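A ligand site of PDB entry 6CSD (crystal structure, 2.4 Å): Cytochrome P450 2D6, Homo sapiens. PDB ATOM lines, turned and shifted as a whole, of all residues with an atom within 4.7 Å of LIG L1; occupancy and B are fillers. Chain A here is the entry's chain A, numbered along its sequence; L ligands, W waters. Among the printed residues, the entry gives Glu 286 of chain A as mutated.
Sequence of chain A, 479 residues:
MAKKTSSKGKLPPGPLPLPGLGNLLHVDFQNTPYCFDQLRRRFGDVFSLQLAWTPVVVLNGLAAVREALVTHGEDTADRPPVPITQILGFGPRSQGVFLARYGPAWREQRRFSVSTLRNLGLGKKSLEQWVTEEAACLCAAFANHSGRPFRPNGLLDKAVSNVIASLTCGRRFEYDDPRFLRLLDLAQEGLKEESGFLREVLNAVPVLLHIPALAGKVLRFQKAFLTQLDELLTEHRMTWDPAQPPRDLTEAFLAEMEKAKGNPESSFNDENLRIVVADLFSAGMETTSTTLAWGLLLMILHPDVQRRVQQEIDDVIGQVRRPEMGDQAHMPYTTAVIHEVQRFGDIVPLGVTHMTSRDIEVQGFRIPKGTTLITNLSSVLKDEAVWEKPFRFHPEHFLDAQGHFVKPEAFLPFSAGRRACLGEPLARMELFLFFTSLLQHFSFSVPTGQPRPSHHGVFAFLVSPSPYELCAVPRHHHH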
ATOM      1  N   LEU A  88      -1.212  -2.526 -25.411  1.00  0.00           N
ATOM      2  CA  LEU A  88      -0.877  -2.354 -24.003  1.00  0.00           C
ATOM      3  C   LEU A  88      -2.037  -1.808 -23.189  1.00  0.00           C
ATOM      4  O   LEU A  88      -1.842  -1.431 -22.033  1.00  0.00           O
ATOM      5  CB  LEU A  88       0.348  -1.431 -23.869  1.00  0.00           C
ATOM      6  CG  LEU A  88       1.575  -1.687 -24.751  1.00  0.00           C
ATOM      7  CD1 LEU A  88       2.719  -0.750 -24.373  1.00  0.00           C
ATOM      8  CD2 LEU A  88       2.040  -3.132 -24.704  1.00  0.00           C
ATOM      9  N   PHE A  90      -4.090   0.900 -24.173  1.00  0.00           N
ATOM     10  CA  PHE A  90      -4.240   2.338 -24.315  1.00  0.00           C
ATOM     11  C   PHE A  90      -5.606   2.681 -24.901  1.00  0.00           C
ATOM     12  O   PHE A  90      -6.059   2.051 -25.861  1.00  0.00           O
ATOM     13  CB  PHE A  90      -3.127   2.914 -25.208  1.00  0.00           C
ATOM     14  CG  PHE A  90      -1.846   3.230 -24.477  1.00  0.00           C
ATOM     15  CD1 PHE A  90      -1.046   2.205 -23.964  1.00  0.00           C
ATOM     16  CD2 PHE A  90      -1.432   4.545 -24.300  1.00  0.00           C
ATOM     17  CE1 PHE A  90       0.143   2.487 -23.309  1.00  0.00           C
ATOM     18  CE2 PHE A  90      -0.249   4.849 -23.647  1.00  0.00           C
ATOM     19  CZ  PHE A  90       0.548   3.805 -23.143  1.00  0.00           C
ATOM     20  N   PHE A  98       3.686   9.529 -20.845  1.00  0.00           N
ATOM     21  CA  PHE A  98       4.772   9.724 -21.788  1.00  0.00           C
ATOM     22  C   PHE A  98       4.261   9.772 -23.231  1.00  0.00           C
ATOM     23  O   PHE A  98       4.567  10.713 -23.968  1.00  0.00           O
ATOM     24  CB  PHE A  98       5.821   8.617 -21.602  1.00  0.00           C
ATOM     25  CG  PHE A  98       7.068   8.838 -22.369  1.00  0.00           C
ATOM     26  CD1 PHE A  98       8.076   9.650 -21.869  1.00  0.00           C
ATOM     27  CD2 PHE A  98       7.258   8.214 -23.593  1.00  0.00           C
ATOM     28  CE1 PHE A  98       9.236   9.860 -22.602  1.00  0.00           C
ATOM     29  CE2 PHE A  98       8.435   8.410 -24.324  1.00  0.00           C
ATOM     30  CZ  PHE A  98       9.414   9.229 -23.826  1.00  0.00           C
ATOM     31  N   LEU A  99       3.478   8.778 -23.658  1.00  0.00           N
ATOM     32  CA  LEU A  99       2.935   8.764 -25.010  1.00  0.00           C
ATOM     33  C   LEU A  99       1.537   9.366 -25.098  1.00  0.00           C
ATOM     34  O   LEU A  99       0.904   9.298 -26.154  1.00  0.00           O
ATOM     35  CB  LEU A  99       2.896   7.331 -25.559  1.00  0.00           C
ATOM     36  CG  LEU A  99       4.211   6.547 -25.639  1.00  0.00           C
ATOM     37  CD1 LEU A  99       3.943   5.066 -25.887  1.00  0.00           C
ATOM     38  CD2 LEU A  99       5.187   7.112 -26.706  1.00  0.00           C
ATOM     39  N   GLY A 190      11.954  -4.062 -23.436  1.00  0.00           N
ATOM     40  CA  GLY A 190      10.805  -3.297 -23.901  1.00  0.00           C
ATOM     41  C   GLY A 190      11.158  -1.904 -24.382  1.00  0.00           C
ATOM     42  O   GLY A 190      10.523  -1.384 -25.306  1.00  0.00           O
ATOM     43  N   LEU A 191      12.170  -1.286 -23.765  1.00  0.00           N
ATOM     44  CA  LEU A 191      12.731  -0.051 -24.302  1.00  0.00           C
ATOM     45  C   LEU A 191      13.292  -0.258 -25.716  1.00  0.00           C
ATOM     46  O   LEU A 191      13.065   0.566 -26.602  1.00  0.00           O
ATOM     47  CB  LEU A 191      13.831   0.474 -23.355  1.00  0.00           C
ATOM     48  CG  LEU A 191      14.492   1.769 -23.800  1.00  0.00           C
ATOM     49  CD1 LEU A 191      13.466   2.902 -23.770  1.00  0.00           C
ATOM     50  CD2 LEU A 191      15.668   2.089 -22.890  1.00  0.00           C
ATOM     51  N   GLU A 194      10.775   0.027 -28.478  1.00  0.00           N
ATOM     52  CA  GLU A 194      10.202   1.334 -28.779  1.00  0.00           C
ATOM     53  C   GLU A 194      10.875   1.947 -30.003  1.00  0.00           C
ATOM     54  O   GLU A 194      10.246   2.728 -30.738  1.00  0.00           O
ATOM     55  CB  GLU A 194      10.336   2.251 -27.560  1.00  0.00           C
ATOM     56  CG  GLU A 194       9.595   3.555 -27.667  1.00  0.00           C
ATOM     57  CD  GLU A 194       8.101   3.422 -27.366  1.00  0.00           C
ATOM     58  OE1 GLU A 194       7.607   2.283 -27.240  1.00  0.00           O
ATOM     59  OE2 GLU A 194       7.439   4.461 -27.262  1.00  0.00           O
ATOM     60  N   GLN A 222       7.336  -5.438 -23.933  1.00  0.00           N
ATOM     61  CA  GLN A 222       6.520  -4.424 -23.281  1.00  0.00           C
ATOM     62  C   GLN A 222       5.259  -5.037 -22.697  1.00  0.00           C
ATOM     63  O   GLN A 222       4.819  -4.654 -21.606  1.00  0.00           O
ATOM     64  CB  GLN A 222       6.161  -3.303 -24.255  1.00  0.00           C
ATOM     65  CG  GLN A 222       7.287  -2.340 -24.560  1.00  0.00           C
ATOM     66  CD  GLN A 222       6.869  -1.246 -25.517  1.00  0.00           C
ATOM     67  OE1 GLN A 222       5.676  -0.988 -25.713  1.00  0.00           O
ATOM     68  NE2 GLN A 222       7.849  -0.579 -26.130  1.00  0.00           N
ATOM     69  N   ILE A 275      -0.540   1.255 -16.842  1.00  0.00           N
ATOM     70  CA  ILE A 275       0.209   2.079 -17.786  1.00  0.00           C
ATOM     71  C   ILE A 275       0.983   3.167 -17.054  1.00  0.00           C
ATOM     72  O   ILE A 275       2.182   3.357 -17.287  1.00  0.00           O
ATOM     73  CB  ILE A 275      -0.726   2.654 -18.861  1.00  0.00           C
ATOM     74  CG1 ILE A 275      -1.348   1.535 -19.687  1.00  0.00           C
ATOM     75  CG2 ILE A 275       0.049   3.604 -19.772  1.00  0.00           C
ATOM     76  CD1 ILE A 275      -2.425   2.032 -20.618  1.00  0.00           C
ATOM     77  N   ALA A 278       3.761   1.735 -14.975  1.00  0.00           N
ATOM     78  CA  ALA A 278       4.825   1.265 -15.874  1.00  0.00           C
ATOM     79  C   ALA A 278       5.644   2.431 -16.430  1.00  0.00           C
ATOM     80  O   ALA A 278       6.881   2.379 -16.435  1.00  0.00           O
ATOM     81  CB  ALA A 278       4.216   0.460 -17.026  1.00  0.00           C
ATOM     82  N   ASP A 279       4.958   3.438 -16.967  1.00  0.00           N
ATOM     83  CA  ASP A 279       5.524   4.710 -17.391  1.00  0.00           C
ATOM     84  C   ASP A 279       6.571   5.246 -16.409  1.00  0.00           C
ATOM     85  O   ASP A 279       7.753   5.406 -16.753  1.00  0.00           O
ATOM     86  CB  ASP A 279       4.359   5.707 -17.524  1.00  0.00           C
ATOM     87  CG  ASP A 279       4.591   6.746 -18.574  1.00  0.00           C
ATOM     88  OD1 ASP A 279       3.623   7.087 -19.295  1.00  0.00           O
ATOM     89  OD2 ASP A 279       5.736   7.252 -18.663  1.00  0.00           O
ATOM     90  N   SER A 282       9.485   2.487 -15.544  1.00  0.00           N
ATOM     91  CA  SER A 282      10.463   2.302 -16.608  1.00  0.00           C
ATOM     92  C   SER A 282      11.274   3.559 -16.841  1.00  0.00           C
ATOM     93  O   SER A 282      12.485   3.496 -17.028  1.00  0.00           O
ATOM     94  CB  SER A 282       9.769   1.842 -17.890  1.00  0.00           C
ATOM     95  OG  SER A 282       8.958   2.860 -18.450  1.00  0.00           O
ATOM     96  N   ALA A 283      10.621   4.730 -16.790  1.00  0.00           N
ATOM     97  CA  ALA A 283      11.363   5.973 -16.968  1.00  0.00           C
ATOM     98  C   ALA A 283      12.360   6.174 -15.826  1.00  0.00           C
ATOM     99  O   ALA A 283      13.520   6.526 -16.051  1.00  0.00           O
ATOM    100  CB  ALA A 283      10.396   7.154 -17.063  1.00  0.00           C
ATOM    101  N   GLU A 286      15.776   3.535 -16.640  1.00  0.00           N
ATOM    102  CA  GLU A 286      16.662   3.664 -17.787  1.00  0.00           C
ATOM    103  C   GLU A 286      17.339   5.014 -17.905  1.00  0.00           C
ATOM    104  O   GLU A 286      18.348   5.117 -18.612  1.00  0.00           O
ATOM    105  CB  GLU A 286      15.862   3.352 -19.052  1.00  0.00           C
ATOM    106  CG  GLU A 286      15.470   1.894 -19.156  1.00  0.00           C
ATOM    107  CD  GLU A 286      13.988   1.693 -19.410  1.00  0.00           C
ATOM    108  OE1 GLU A 286      13.402   2.488 -20.169  1.00  0.00           O
ATOM    109  OE2 GLU A 286      13.412   0.727 -18.887  1.00  0.00           O
ATOM    110  N   THR A 287      16.832   6.047 -17.267  1.00  0.00           N
ATOM    111  CA  THR A 287      17.362   7.386 -17.523  1.00  0.00           C
ATOM    112  C   THR A 287      18.494   7.733 -16.582  1.00  0.00           C
ATOM    113  O   THR A 287      19.609   8.003 -17.030  1.00  0.00           O
ATOM    114  CB  THR A 287      16.243   8.407 -17.349  1.00  0.00           C
ATOM    115  OG1 THR A 287      15.642   8.182 -16.064  1.00  0.00           O
ATOM    116  CG2 THR A 287      15.216   8.247 -18.452  1.00  0.00           C
ATOM    117  N   VAL A 348      19.249  11.514 -24.315  1.00  0.00           N
ATOM    118  CA  VAL A 348      18.138  11.458 -25.269  1.00  0.00           C
ATOM    119  C   VAL A 348      18.436  12.430 -26.401  1.00  0.00           C
ATOM    120  O   VAL A 348      17.902  13.551 -26.391  1.00  0.00           O
ATOM    121  CB  VAL A 348      16.799  11.810 -24.584  1.00  0.00           C
ATOM    122  CG1 VAL A 348      15.641  11.422 -25.472  1.00  0.00           C
ATOM    123  CG2 VAL A 348      16.663  11.147 -23.284  1.00  0.00           C
ATOM    124  N   CYS A 421      10.383  16.841 -19.147  1.00  0.00           N
ATOM    125  CA  CYS A 421      10.489  15.674 -18.274  1.00  0.00           C
ATOM    126  C   CYS A 421       9.944  15.975 -16.897  1.00  0.00           C
ATOM    127  O   CYS A 421      10.445  16.877 -16.214  1.00  0.00           O
ATOM    128  CB  CYS A 421      11.957  15.274 -18.160  1.00  0.00           C
ATOM    129  SG  CYS A 421      12.197  13.918 -16.973  1.00  0.00           S
ATOM    130  N   PHE A 461      17.128   4.979 -28.896  1.00  0.00           N
ATOM    131  CA  PHE A 461      16.315   6.044 -28.323  1.00  0.00           C
ATOM    132  C   PHE A 461      17.064   6.727 -27.175  1.00  0.00           C
ATOM    133  O   PHE A 461      17.188   7.952 -27.141  1.00  0.00           O
ATOM    134  CB  PHE A 461      14.954   5.503 -27.848  1.00  0.00           C
ATOM    135  CG  PHE A 461      14.172   6.493 -27.062  1.00  0.00           C
ATOM    136  CD1 PHE A 461      13.683   7.630 -27.659  1.00  0.00           C
ATOM    137  CD2 PHE A 461      13.961   6.315 -25.714  1.00  0.00           C
ATOM    138  CE1 PHE A 461      12.967   8.550 -26.938  1.00  0.00           C
ATOM    139  CE2 PHE A 461      13.253   7.236 -24.999  1.00  0.00           C
ATOM    140  CZ  PHE A 461      12.761   8.353 -25.606  1.00  0.00           C
ATOM    141  N   LEU A 462      17.610   5.932 -26.272  1.00  0.00           N
ATOM    142  CA  LEU A 462      18.460   6.387 -25.184  1.00  0.00           C
ATOM    143  C   LEU A 462      19.899   5.973 -25.499  1.00  0.00           C
ATOM    144  O   LEU A 462      20.133   4.850 -25.935  1.00  0.00           O
ATOM    145  CB  LEU A 462      17.970   5.748 -23.883  1.00  0.00           C
ATOM    146  CG  LEU A 462      18.109   6.523 -22.597  1.00  0.00           C
ATOM    147  CD1 LEU A 462      16.957   7.506 -22.457  1.00  0.00           C
ATOM    148  CD2 LEU A 462      18.036   5.512 -21.536  1.00  0.00           C
HETATM  149  N1  LIG L   1       7.482   2.486 -22.726  1.00  0.00           N
HETATM  150  N2  LIG L   1       7.614   4.637 -20.216  1.00  0.00           N
HETATM  151  C1  LIG L   1       5.485   2.228 -24.131  1.00  0.00           C
HETATM  152  C2  LIG L   1       9.920   3.677 -22.430  1.00  0.00           C
HETATM  153  C3  LIG L   1       9.928   4.628 -23.427  1.00  0.00           C
HETATM  154  C4  LIG L   1      10.718   5.748 -23.284  1.00  0.00           C
HETATM  155  C5  LIG L   1      11.492   5.904 -22.157  1.00  0.00           C
HETATM  156  C6  LIG L   1      10.654   3.852 -21.268  1.00  0.00           C
HETATM  157  C7  LIG L   1      13.020  10.124 -20.579  1.00  0.00           C
HETATM  158  C8  LIG L   1      11.233   8.105 -20.451  1.00  0.00           C
HETATM  159  C9  LIG L   1       4.620   2.470 -20.081  1.00  0.00           C
HETATM  160  C10 LIG L   1       5.406   2.101 -21.335  1.00  0.00           C
HETATM  161  C11 LIG L   1       6.771   2.792 -21.460  1.00  0.00           C
HETATM  162  C12 LIG L   1       6.813   2.925 -23.957  1.00  0.00           C
HETATM  163  S1  LIG L   1       4.346   2.571 -22.773  1.00  0.00           S
HETATM  164  S2  LIG L   1       9.076   2.159 -22.696  1.00  0.00           S
HETATM  165  C13 LIG L   1      11.444   4.972 -21.125  1.00  0.00           C
HETATM  166  O1  LIG L   1      12.425   6.934 -22.182  1.00  0.00           O
HETATM  167  C14 LIG L   1      12.271   8.022 -21.347  1.00  0.00           C
HETATM  168  C15 LIG L   1      13.184   9.061 -21.428  1.00  0.00           C
HETATM  169  N3  LIG L   1      12.025  10.218 -19.689  1.00  0.00           N
HETATM  170  C16 LIG L   1      11.157   9.216 -19.640  1.00  0.00           C
HETATM  171  O2  LIG L   1       9.417   1.698 -24.012  1.00  0.00           O
HETATM  172  O3  LIG L   1       9.318   1.319 -21.567  1.00  0.00           O
HETATM  173  C17 LIG L   1       6.792   4.299 -21.190  1.00  0.00           C
HETATM  174  O4  LIG L   1       7.792   5.993 -19.902  1.00  0.00           O
HETATM  175  O5  LIG L   1       6.132   5.119 -21.839  1.00  0.00           O
HETATM  176  C18 LIG L   1       5.617   0.584 -21.365  1.00  0.00           C
HETATM  177  C1  LG2 L   2       9.771  13.129 -20.663  1.00  0.00           C
HETATM  178  C2  LG2 L   2      14.659  13.310 -20.364  1.00  0.00           C
HETATM  179  C3  LG2 L   2      14.434  10.966 -16.129  1.00  0.00           C
HETATM  180  C4  LG2 L   2       9.646  10.568 -16.587  1.00  0.00           C
HETATM  181  C5  LG2 L   2      11.107  13.360 -20.958  1.00  0.00           C
HETATM  182  C6  LG2 L   2      11.593  14.048 -22.137  1.00  0.00           C
HETATM  183  C7  LG2 L   2      12.946  14.110 -22.064  1.00  0.00           C
HETATM  184  C8  LG2 L   2      13.359  13.467 -20.818  1.00  0.00           C
HETATM  185  C9  LG2 L   2      13.876  14.746 -23.139  1.00  0.00           C
HETATM  186  C10 LG2 L   2      10.707  14.566 -23.279  1.00  0.00           C
HETATM  187  C11 LG2 L   2      10.102  15.932 -23.019  1.00  0.00           C
HETATM  188  C12 LG2 L   2       9.435  16.348 -24.318  1.00  0.00           C
HETATM  189  O1  LG2 L   2       8.372  15.779 -24.711  1.00  0.00           O
HETATM  190  O2  LG2 L   2       9.981  17.255 -24.991  1.00  0.00           O
HETATM  191  C13 LG2 L   2      15.048  12.720 -19.182  1.00  0.00           C
HETATM  192  C14 LG2 L   2      16.378  12.650 -18.602  1.00  0.00           C
HETATM  193  C15 LG2 L   2      16.288  11.991 -17.422  1.00  0.00           C
HETATM  194  C16 LG2 L   2      14.914  11.632 -17.225  1.00  0.00           C
HETATM  195  C17 LG2 L   2      17.644  13.251 -19.313  1.00  0.00           C
HETATM  196  C18 LG2 L   2      17.338  11.589 -16.354  1.00  0.00           C
HETATM  197  C19 LG2 L   2      18.623  11.880 -16.405  1.00  0.00           C
HETATM  198  C20 LG2 L   2      13.112  10.691 -15.861  1.00  0.00           C
HETATM  199  C21 LG2 L   2      12.604  10.134 -14.626  1.00  0.00           C
HETATM  200  C22 LG2 L   2      11.263  10.009 -14.782  1.00  0.00           C
HETATM  201  C23 LG2 L   2      10.917  10.518 -16.094  1.00  0.00           C
HETATM  202  C24 LG2 L   2      13.494   9.747 -13.414  1.00  0.00           C
HETATM  203  C25 LG2 L   2      10.180   9.484 -13.806  1.00  0.00           C
HETATM  204  C26 LG2 L   2      10.330   9.583 -12.486  1.00  0.00           C
HETATM  205  C27 LG2 L   2       9.243  11.227 -17.720  1.00  0.00           C
HETATM  206  C28 LG2 L   2       7.876  11.343 -18.171  1.00  0.00           C
HETATM  207  C29 LG2 L   2       7.891  12.061 -19.299  1.00  0.00           C
HETATM  208  C30 LG2 L   2       9.281  12.403 -19.595  1.00  0.00           C
HETATM  209  C31 LG2 L   2       6.657  10.733 -17.436  1.00  0.00           C
HETATM  210  C32 LG2 L   2       6.667  12.466 -20.131  1.00  0.00           C
HETATM  211  C33 LG2 L   2       6.270  13.875 -19.696  1.00  0.00           C
HETATM  212  C34 LG2 L   2       5.056  14.351 -20.480  1.00  0.00           C
HETATM  213  O3  LG2 L   2       4.325  15.246 -19.980  1.00  0.00           O
HETATM  214  O4  LG2 L   2       4.826  13.831 -21.618  1.00  0.00           O
HETATM  215  N1  LG2 L   2      12.209  13.030 -20.180  1.00  0.00           N
HETATM  216  N2  LG2 L   2      14.200  12.078 -18.315  1.00  0.00           N
HETATM  217  N3  LG2 L   2      12.074  10.905 -16.736  1.00  0.00           N
HETATM  218  N4  LG2 L   2      10.057  11.884 -18.593  1.00  0.00           N
HETATM  219 FE1  LG2 L   2      12.132  12.036 -18.403  1.00  0.00          FE
HETATM  220  O   HOH W   1       3.400   5.738 -21.386  1.00  0.00           O
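FE1 of LG2 L2 is bound by SG of Cys 421, 2.4 Å away.
O of Asp 279 lies within hydrogen-bond range of O4 of LIG L1, at 3.2 Å.
The side-chain hydroxyl of Ser 282 sits at hydrogen-bond distance from a nitrogen (N2) of LIG L1 (2.8 Å).
O4 of LIG L1 sits at hydrogen-bond distance from OD2 of Asp 279.
An oxygen (O2) of LIG L1 is in hydrogen-bond range of the side-chain amide nitrogen (NE2) of Gln 222, at 3.5 Å.
N3 of LIG L1 is bound to FE1 of LG2 L2, at 2.2 Å.
The side-chain carboxylate (OD1) of Asp 279 lies within hydrogen-bond range of the backbone NH (N) of Phe 98 (2.9 Å).
The backbone carbonyl oxygen of Asp 279 lies within hydrogen-bond range of the side-chain hydroxyl of Ser 282, at 3.3 Å.
The backbone carbonyl oxygen of Ala 278 is in hydrogen-bond range of the side-chain hydroxyl of Ser 282 (2.9 Å).
The side-chain carboxylate of Glu 194 is in hydrogen-bond range of the side-chain amide nitrogen of Gln 222, 3.1 Å away.
O of Gly 190 is in hydrogen-bond range of NE2 of Gln 222 (2.9 Å).
O of Ala 283 lies within hydrogen-bond range of OG1 of Thr 287.
CE1 of Phe 98 touches C8 of LIG L1 (3.4 Å).
CD1 of Leu 99 touches C1 of LIG L1 (3.7 Å).
O of Gly 190 touches O2 of LIG L1 (3.5 Å).
Leu 191 touches LIG L1 (CA to O2, 3.8 Å).
OE1 of Glu 194 touches C12 of LIG L1, 3.4 Å away.
Ile 275 touches LIG L1.
CB of Ala 278 touches C9 of LIG L1, at 3.7 Å.
CB of Ala 283 touches C16 of LIG L1 (3.4 Å).
Glu 286 touches LIG L1.
CG2 of Thr 287 touches C7 of LIG L1, at 3.6 Å.
CE2 of Phe 461 touches O1 of LIG L1 (3.0 Å).
Hydrophobic or aromatic side chains within 4 Å of LIG L1: Phe 98, Leu 99, Leu 191, Ala 278, Ala 283 and Phe 461.
Within 4 Å of LIG L1: Phe 98, Leu 99, Gly 190, Leu 191, Glu 194, Gln 222, Ile 275, Ala 278, Asp 279, Ser 282, Ala 283, Glu 286, Thr 287 and Phe 461.
Water W1 lies within hydrogen-bond range of the side-chain carboxylate (OD1) of Asp 279 and an oxygen (O5) of LIG L1.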
